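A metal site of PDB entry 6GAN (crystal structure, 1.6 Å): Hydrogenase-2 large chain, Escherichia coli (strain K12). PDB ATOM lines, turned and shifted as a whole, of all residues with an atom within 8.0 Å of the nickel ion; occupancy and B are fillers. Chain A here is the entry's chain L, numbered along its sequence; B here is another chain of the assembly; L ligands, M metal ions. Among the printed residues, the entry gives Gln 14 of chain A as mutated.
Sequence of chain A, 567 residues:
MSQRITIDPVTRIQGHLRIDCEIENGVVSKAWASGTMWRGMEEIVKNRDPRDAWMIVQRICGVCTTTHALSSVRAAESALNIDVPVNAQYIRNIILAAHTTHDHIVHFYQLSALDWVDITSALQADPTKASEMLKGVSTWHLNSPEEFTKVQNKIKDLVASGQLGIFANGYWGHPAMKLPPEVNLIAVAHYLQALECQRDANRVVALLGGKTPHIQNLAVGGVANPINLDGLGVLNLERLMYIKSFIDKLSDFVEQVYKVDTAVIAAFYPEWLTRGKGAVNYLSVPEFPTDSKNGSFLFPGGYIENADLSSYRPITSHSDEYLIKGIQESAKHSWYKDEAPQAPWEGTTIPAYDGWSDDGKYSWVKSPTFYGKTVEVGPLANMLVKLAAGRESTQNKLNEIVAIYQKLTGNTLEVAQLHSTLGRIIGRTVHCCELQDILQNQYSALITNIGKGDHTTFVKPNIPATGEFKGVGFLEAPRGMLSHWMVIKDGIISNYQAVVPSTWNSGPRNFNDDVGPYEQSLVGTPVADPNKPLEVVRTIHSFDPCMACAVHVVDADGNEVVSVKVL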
ATOM      1  N   GLN A  14       8.622 -31.795  18.263  1.00  0.00           N
ATOM      2  CA  GLN A  14       8.084 -32.439  19.438  1.00  0.00           C
ATOM      3  C   GLN A  14       6.864 -33.255  19.042  1.00  0.00           C
ATOM      4  O   GLN A  14       5.933 -32.736  18.390  1.00  0.00           O
ATOM      5  CB  GLN A  14       7.697 -31.406  20.492  1.00  0.00           C
ATOM      6  CG  GLN A  14       7.356 -32.058  21.834  1.00  0.00           C
ATOM      7  CD  GLN A  14       6.100 -32.906  21.867  1.00  0.00           C
ATOM      8  OE1 GLN A  14       5.116 -32.572  21.236  1.00  0.00           O
ATOM      9  NE2 GLN A  14       6.117 -34.022  22.634  1.00  0.00           N
ATOM     10  N   GLN A  58       1.224 -28.186  33.045  1.00  0.00           N
ATOM     11  CA  GLN A  58       2.587 -27.880  32.556  1.00  0.00           C
ATOM     12  C   GLN A  58       3.117 -29.071  31.764  1.00  0.00           C
ATOM     13  O   GLN A  58       3.815 -28.915  30.766  1.00  0.00           O
ATOM     14  CB  GLN A  58       3.531 -27.559  33.716  1.00  0.00           C
ATOM     15  CG  GLN A  58       4.871 -27.095  33.182  1.00  0.00           C
ATOM     16  CD  GLN A  58       5.875 -26.515  34.164  1.00  0.00           C
ATOM     17  OE1 GLN A  58       6.822 -25.789  33.705  1.00  0.00           O
ATOM     18  NE2 GLN A  58       5.786 -26.906  35.468  1.00  0.00           N
ATOM     19  N   ILE A  60       1.554 -30.788  29.665  1.00  0.00           N
ATOM     20  CA  ILE A  60       1.186 -30.817  28.255  1.00  0.00           C
ATOM     21  C   ILE A  60       2.454 -30.947  27.416  1.00  0.00           C
ATOM     22  O   ILE A  60       2.468 -31.684  26.399  1.00  0.00           O
ATOM     23  CB  ILE A  60       0.309 -29.645  27.892  1.00  0.00           C
ATOM     24  CG1 ILE A  60      -1.114 -29.928  28.449  1.00  0.00           C
ATOM     25  CG2 ILE A  60       0.276 -29.428  26.392  1.00  0.00           C
ATOM     26  CD1 ILE A  60      -1.987 -28.691  28.376  1.00  0.00           C
ATOM     27  N   CYS A  61       3.507 -30.236  27.800  1.00  0.00           N
ATOM     28  CA  CYS A  61       4.719 -30.213  26.943  1.00  0.00           C
ATOM     29  C   CYS A  61       5.971 -29.896  27.754  1.00  0.00           C
ATOM     30  O   CYS A  61       5.958 -28.998  28.592  1.00  0.00           O
ATOM     31  CB  CYS A  61       4.527 -29.207  25.805  1.00  0.00           C
ATOM     32  SG  CYS A  61       5.853 -29.256  24.558  1.00  0.00           S
ATOM     33  N   GLY A  62       7.044 -30.663  27.492  1.00  0.00           N
ATOM     34  CA  GLY A  62       8.343 -30.453  28.081  1.00  0.00           C
ATOM     35  C   GLY A  62       9.346 -29.730  27.181  1.00  0.00           C
ATOM     36  O   GLY A  62      10.378 -29.309  27.683  1.00  0.00           O
ATOM     37  N   VAL A  63       9.027 -29.528  25.888  1.00  0.00           N
ATOM     38  CA  VAL A  63       9.832 -28.671  25.043  1.00  0.00           C
ATOM     39  C   VAL A  63       9.467 -27.227  25.409  1.00  0.00           C
ATOM     40  O   VAL A  63      10.321 -26.467  25.830  1.00  0.00           O
ATOM     41  CB  VAL A  63       9.573 -28.975  23.578  1.00  0.00           C
ATOM     42  CG1 VAL A  63      10.292 -27.983  22.676  1.00  0.00           C
ATOM     43  CG2 VAL A  63      10.023 -30.374  23.286  1.00  0.00           C
ATOM     44  N   CYS A  64       8.183 -26.868  25.242  1.00  0.00           N
ATOM     45  CA  CYS A  64       7.676 -25.579  25.733  1.00  0.00           C
ATOM     46  C   CYS A  64       7.270 -25.697  27.178  1.00  0.00           C
ATOM     47  O   CYS A  64       6.179 -25.276  27.576  1.00  0.00           O
ATOM     48  CB  CYS A  64       6.577 -24.945  24.835  1.00  0.00           C
ATOM     49  SG  CYS A  64       5.108 -25.987  24.730  1.00  0.00           S
ATOM     50  N   THR A  65       8.182 -26.229  27.976  1.00  0.00           N
ATOM     51  CA  THR A  65       8.038 -26.195  29.426  1.00  0.00           C
ATOM     52  C   THR A  65       7.951 -24.715  29.839  1.00  0.00           C
ATOM     53  O   THR A  65       8.312 -23.841  29.058  1.00  0.00           O
ATOM     54  CB  THR A  65       9.112 -26.994  30.183  1.00  0.00           C
ATOM     55  OG1 THR A  65       8.767 -27.073  31.583  1.00  0.00           O
ATOM     56  CG2 THR A  65      10.482 -26.304  30.029  1.00  0.00           C
ATOM     57  N   THR A  67       5.428 -22.789  29.729  1.00  0.00           N
ATOM     58  CA  THR A  67       4.400 -22.018  29.092  1.00  0.00           C
ATOM     59  C   THR A  67       3.009 -22.377  29.568  1.00  0.00           C
ATOM     60  O   THR A  67       2.177 -21.477  29.838  1.00  0.00           O
ATOM     61  CB  THR A  67       4.478 -22.099  27.544  1.00  0.00           C
ATOM     62  OG1 THR A  67       4.153 -23.429  27.088  1.00  0.00           O
ATOM     63  CG2 THR A  67       5.861 -21.675  27.036  1.00  0.00           C
ATOM     64  N   HIS A  68       2.699 -23.659  29.680  1.00  0.00           N
ATOM     65  CA  HIS A  68       1.373 -24.047  30.151  1.00  0.00           C
ATOM     66  C   HIS A  68       1.193 -23.827  31.645  1.00  0.00           C
ATOM     67  O   HIS A  68       0.074 -23.550  32.084  1.00  0.00           O
ATOM     68  CB  HIS A  68       1.144 -25.548  29.821  1.00  0.00           C
ATOM     69  CG  HIS A  68       1.041 -25.795  28.367  1.00  0.00           C
ATOM     70  ND1 HIS A  68      -0.075 -25.469  27.658  1.00  0.00           N
ATOM     71  CD2 HIS A  68       1.946 -26.272  27.474  1.00  0.00           C
ATOM     72  CE1 HIS A  68       0.120 -25.741  26.382  1.00  0.00           C
ATOM     73  NE2 HIS A  68       1.342 -26.218  26.238  1.00  0.00           N
ATOM     74  N   HIS A  99      13.524 -19.183  28.814  1.00  0.00           N
ATOM     75  CA  HIS A  99      13.105 -20.429  28.264  1.00  0.00           C
ATOM     76  C   HIS A  99      12.992 -20.391  26.734  1.00  0.00           C
ATOM     77  O   HIS A  99      13.402 -21.229  26.031  1.00  0.00           O
ATOM     78  CB  HIS A  99      11.717 -20.885  28.756  1.00  0.00           C
ATOM     79  CG  HIS A  99      11.239 -22.027  27.942  1.00  0.00           C
ATOM     80  ND1 HIS A  99      11.699 -23.296  28.143  1.00  0.00           N
ATOM     81  CD2 HIS A  99      10.522 -22.059  26.800  1.00  0.00           C
ATOM     82  CE1 HIS A  99      11.213 -24.082  27.203  1.00  0.00           C
ATOM     83  NE2 HIS A  99      10.496 -23.355  26.380  1.00  0.00           N
ATOM     84  N   ASP A 103      14.597 -22.446  23.662  1.00  0.00           N
ATOM     85  CA  ASP A 103      13.694 -23.136  22.757  1.00  0.00           C
ATOM     86  C   ASP A 103      14.016 -22.790  21.303  1.00  0.00           C
ATOM     87  O   ASP A 103      14.226 -23.700  20.466  1.00  0.00           O
ATOM     88  CB  ASP A 103      12.250 -22.757  23.194  1.00  0.00           C
ATOM     89  CG  ASP A 103      11.206 -23.726  22.745  1.00  0.00           C
ATOM     90  OD1 ASP A 103      11.371 -24.273  21.611  1.00  0.00           O
ATOM     91  OD2 ASP A 103      10.158 -23.844  23.475  1.00  0.00           O
ATOM     92  N   ALA A 477       3.681 -17.745  23.510  1.00  0.00           N
ATOM     93  CA  ALA A 477       4.626 -18.811  23.644  1.00  0.00           C
ATOM     94  C   ALA A 477       5.578 -18.864  22.498  1.00  0.00           C
ATOM     95  O   ALA A 477       5.389 -18.171  21.473  1.00  0.00           O
ATOM     96  CB  ALA A 477       3.876 -20.152  23.744  1.00  0.00           C
ATOM     97  N   PRO A 478       6.604 -19.723  22.599  1.00  0.00           N
ATOM     98  CA  PRO A 478       7.580 -19.762  21.500  1.00  0.00           C
ATOM     99  C   PRO A 478       6.976 -20.103  20.144  1.00  0.00           C
ATOM    100  O   PRO A 478       7.430 -19.595  19.113  1.00  0.00           O
ATOM    101  CB  PRO A 478       8.545 -20.910  21.942  1.00  0.00           C
ATOM    102  CG  PRO A 478       8.481 -20.883  23.442  1.00  0.00           C
ATOM    103  CD  PRO A 478       7.073 -20.487  23.758  1.00  0.00           C
ATOM    104  N   ARG A 479       5.863 -20.860  20.142  1.00  0.00           N
ATOM    105  CA  ARG A 479       5.207 -21.256  18.907  1.00  0.00           C
ATOM    106  C   ARG A 479       3.978 -20.429  18.609  1.00  0.00           C
ATOM    107  O   ARG A 479       3.362 -20.664  17.598  1.00  0.00           O
ATOM    108  CB  ARG A 479       4.898 -22.765  18.935  1.00  0.00           C
ATOM    109  CG  ARG A 479       6.173 -23.576  18.880  1.00  0.00           C
ATOM    110  CD  ARG A 479       6.062 -24.990  19.389  1.00  0.00           C
ATOM    111  NE  ARG A 479       7.369 -25.624  19.395  1.00  0.00           N
ATOM    112  CZ  ARG A 479       8.308 -25.440  20.326  1.00  0.00           C
ATOM    113  NH1 ARG A 479       8.092 -24.745  21.419  1.00  0.00           N
ATOM    114  NH2 ARG A 479       9.537 -25.910  20.152  1.00  0.00           N
ATOM    115  N   VAL A 500      -3.892 -24.242  21.846  1.00  0.00           N
ATOM    116  CA  VAL A 500      -2.459 -24.137  21.932  1.00  0.00           C
ATOM    117  C   VAL A 500      -1.932 -23.683  20.591  1.00  0.00           C
ATOM    118  O   VAL A 500      -2.571 -23.938  19.583  1.00  0.00           O
ATOM    119  CB  VAL A 500      -1.878 -25.510  22.401  1.00  0.00           C
ATOM    120  CG1 VAL A 500      -0.390 -25.437  22.663  1.00  0.00           C
ATOM    121  CG2 VAL A 500      -2.628 -25.975  23.666  1.00  0.00           C
ATOM    122  N   PRO A 501      -0.773 -23.017  20.501  1.00  0.00           N
ATOM    123  CA  PRO A 501      -0.421 -22.482  19.187  1.00  0.00           C
ATOM    124  C   PRO A 501      -0.279 -23.516  18.083  1.00  0.00           C
ATOM    125  O   PRO A 501      -0.776 -23.283  16.960  1.00  0.00           O
ATOM    126  CB  PRO A 501       0.914 -21.765  19.422  1.00  0.00           C
ATOM    127  CG  PRO A 501       1.351 -22.115  20.801  1.00  0.00           C
ATOM    128  CD  PRO A 501       0.102 -22.452  21.555  1.00  0.00           C
ATOM    129  N   SER A 502       0.339 -24.657  18.349  1.00  0.00           N
ATOM    130  CA  SER A 502       0.377 -25.681  17.292  1.00  0.00           C
ATOM    131  C   SER A 502      -1.015 -26.270  16.966  1.00  0.00           C
ATOM    132  O   SER A 502      -1.144 -26.836  15.868  1.00  0.00           O
ATOM    133  CB  SER A 502       1.330 -26.806  17.673  1.00  0.00           C
ATOM    134  OG  SER A 502       2.696 -26.347  17.644  1.00  0.00           O
ATOM    135  N   ASP A 544       7.777 -25.073  13.602  1.00  0.00           N
ATOM    136  CA  ASP A 544       8.213 -25.578  14.924  1.00  0.00           C
ATOM    137  C   ASP A 544       7.083 -26.440  15.588  1.00  0.00           C
ATOM    138  O   ASP A 544       6.586 -26.142  16.674  1.00  0.00           O
ATOM    139  CB  ASP A 544       8.671 -24.359  15.753  1.00  0.00           C
ATOM    140  CG  ASP A 544       9.300 -24.702  17.049  1.00  0.00           C
ATOM    141  OD1 ASP A 544       9.564 -25.872  17.333  1.00  0.00           O
ATOM    142  OD2 ASP A 544       9.467 -23.705  17.818  1.00  0.00           O
ATOM    143  N   PRO A 545       6.640 -27.495  14.879  1.00  0.00           N
ATOM    144  CA  PRO A 545       5.534 -28.291  15.420  1.00  0.00           C
ATOM    145  C   PRO A 545       5.793 -28.849  16.806  1.00  0.00           C
ATOM    146  O   PRO A 545       6.858 -29.353  17.127  1.00  0.00           O
ATOM    147  CB  PRO A 545       5.342 -29.406  14.392  1.00  0.00           C
ATOM    148  CG  PRO A 545       6.014 -28.943  13.162  1.00  0.00           C
ATOM    149  CD  PRO A 545       7.146 -28.092  13.625  1.00  0.00           C
ATOM    150  N   CYS A 546       4.751 -28.750  17.632  1.00  0.00           N
ATOM    151  CA  CYS A 546       4.762 -29.392  18.935  1.00  0.00           C
ATOM    152  C   CYS A 546       3.423 -30.123  19.081  1.00  0.00           C
ATOM    153  O   CYS A 546       2.382 -29.524  19.315  1.00  0.00           O
ATOM    154  CB  CYS A 546       4.924 -28.312  19.981  1.00  0.00           C
ATOM    155  SG  CYS A 546       5.190 -29.067  21.600  1.00  0.00           S
ATOM    156  N   MET A 547       3.425 -31.457  18.892  1.00  0.00           N
ATOM    157  CA  MET A 547       2.160 -32.159  18.847  1.00  0.00           C
ATOM    158  C   MET A 547       1.593 -32.565  20.205  1.00  0.00           C
ATOM    159  O   MET A 547       0.373 -32.783  20.306  1.00  0.00           O
ATOM    160  CB  MET A 547       2.274 -33.402  17.974  1.00  0.00           C
ATOM    161  CG  MET A 547       2.675 -33.051  16.549  1.00  0.00           C
ATOM    162  SD  MET A 547       1.936 -31.644  15.736  1.00  0.00           S
ATOM    163  CE  MET A 547       0.267 -32.282  15.485  1.00  0.00           C
ATOM    164  N   ALA A 548       2.429 -32.688  21.217  1.00  0.00           N
ATOM    165  CA  ALA A 548       1.905 -32.823  22.603  1.00  0.00           C
ATOM    166  C   ALA A 548       1.134 -31.556  22.973  1.00  0.00           C
ATOM    167  O   ALA A 548       0.030 -31.599  23.530  1.00  0.00           O
ATOM    168  CB  ALA A 548       3.039 -33.062  23.557  1.00  0.00           C
ATOM    169  N   CYS A 549       1.690 -30.425  22.567  1.00  0.00           N
ATOM    170  CA  CYS A 549       0.946 -29.146  22.646  1.00  0.00           C
ATOM    171  C   CYS A 549      -0.309 -29.117  21.810  1.00  0.00           C
ATOM    172  O   CYS A 549      -1.371 -28.737  22.287  1.00  0.00           O
ATOM    173  CB  CYS A 549       1.853 -28.027  22.192  1.00  0.00           C
ATOM    174  SG  CYS A 549       2.822 -27.289  23.547  1.00  0.00           S
ATOM    175  N   ALA A 550      -0.218 -29.514  20.531  1.00  0.00           N
ATOM    176  CA  ALA A 550      -1.342 -29.354  19.642  1.00  0.00           C
ATOM    177  C   ALA A 550      -2.553 -30.140  20.130  1.00  0.00           C
ATOM    178  O   ALA A 550      -3.670 -29.667  19.990  1.00  0.00           O
ATOM    179  CB  ALA A 550      -0.989 -29.853  18.248  1.00  0.00           C
ATOM    180  N   CYS B  22       5.838 -36.073  26.942  1.00  0.00           N
ATOM    181  CA  CYS B  22       5.750 -34.627  26.714  1.00  0.00           C
ATOM    182  C   CYS B  22       7.076 -34.105  26.192  1.00  0.00           C
ATOM    183  O   CYS B  22       7.199 -32.921  25.857  1.00  0.00           O
ATOM    184  CB  CYS B  22       5.354 -33.884  28.006  1.00  0.00           C
ATOM    185  SG  CYS B  22       6.755 -33.670  29.167  1.00  0.00           S
ATOM    186  N   THR B  23       8.097 -34.978  26.121  1.00  0.00           N
ATOM    187  CA  THR B  23       9.454 -34.686  25.648  1.00  0.00           C
ATOM    188  C   THR B  23      10.359 -34.074  26.764  1.00  0.00           C
ATOM    189  O   THR B  23      11.572 -33.917  26.610  1.00  0.00           O
ATOM    190  CB  THR B  23       9.499 -33.910  24.306  1.00  0.00           C
ATOM    191  OG1 THR B  23       8.650 -34.635  23.412  1.00  0.00           O
ATOM    192  CG2 THR B  23      10.932 -33.843  23.700  1.00  0.00           C
HETATM  193 FE1  LIG L   1       3.841 -25.381  22.970  1.00  0.00          FE
HETATM  194  C1  LIG L   1       3.015 -25.378  21.267  1.00  0.00           C
HETATM  195  N1  LIG L   1       2.516 -25.297  20.237  1.00  0.00           N
HETATM  196  C2  LIG L   1       4.955 -23.914  22.518  1.00  0.00           C
HETATM  197  N2  LIG L   1       5.560 -22.986  22.258  1.00  0.00           N
HETATM  198  C3  LIG L   1       2.773 -24.181  23.683  1.00  0.00           C
HETATM  199  O1  LIG L   1       1.994 -23.408  24.117  1.00  0.00           O
HETATM  200 NI    NI M   1       5.133 -27.612  23.243  1.00  0.00          NI
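FE1 of the ligand is bound by SG of Cys 64 (2.3 Å).
FE1 of the ligand is bound by SG of Cys 549 (2.2 Å).
A nitrogen (N2) of the ligand is in hydrogen-bond range of the backbone NH of Arg 479 (3.0 Å).
NH1 of Arg 479 is in hydrogen-bond range of N2 of the ligand.
A nitrogen (N1) of the ligand lies within hydrogen-bond range of the backbone NH (N) of Ser 502 (3.0 Å).
OG of Ser 502 sits at hydrogen-bond distance from N1 of the ligand, at 2.8 Å.
The nickel ion is bound by SG of Cys 546 (2.2 Å), SG of Cys 64 (2.2 Å), SG of Cys 61 (2.2 Å) and SG of Cys 549 (2.4 Å).
Of the 27 residues printed, 4 come within 4 Å of the nickel ion.
The nearest printed residue that does not touch the nickel ion is Arg 479 (4.5 Å).
The side-chain sulfur (SG) of Cys 546 sits close to the side-chain amide oxygen (OE1) of Gln 14.
The side-chain hydroxyl (OG) of Ser 502 sits at hydrogen-bond distance from the backbone NH (N) of Cys 546 (3.2 Å).
O of Cys 64 sits at hydrogen-bond distance from OG1 of Thr 67, at 2.8 Å.
The side-chain sulfur (SG) of Cys 61 lies close to the backbone NH (N) of Val 63.
The side-chain sulfur of Cys 549 sits close to a ring nitrogen (NE2) of His 68.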
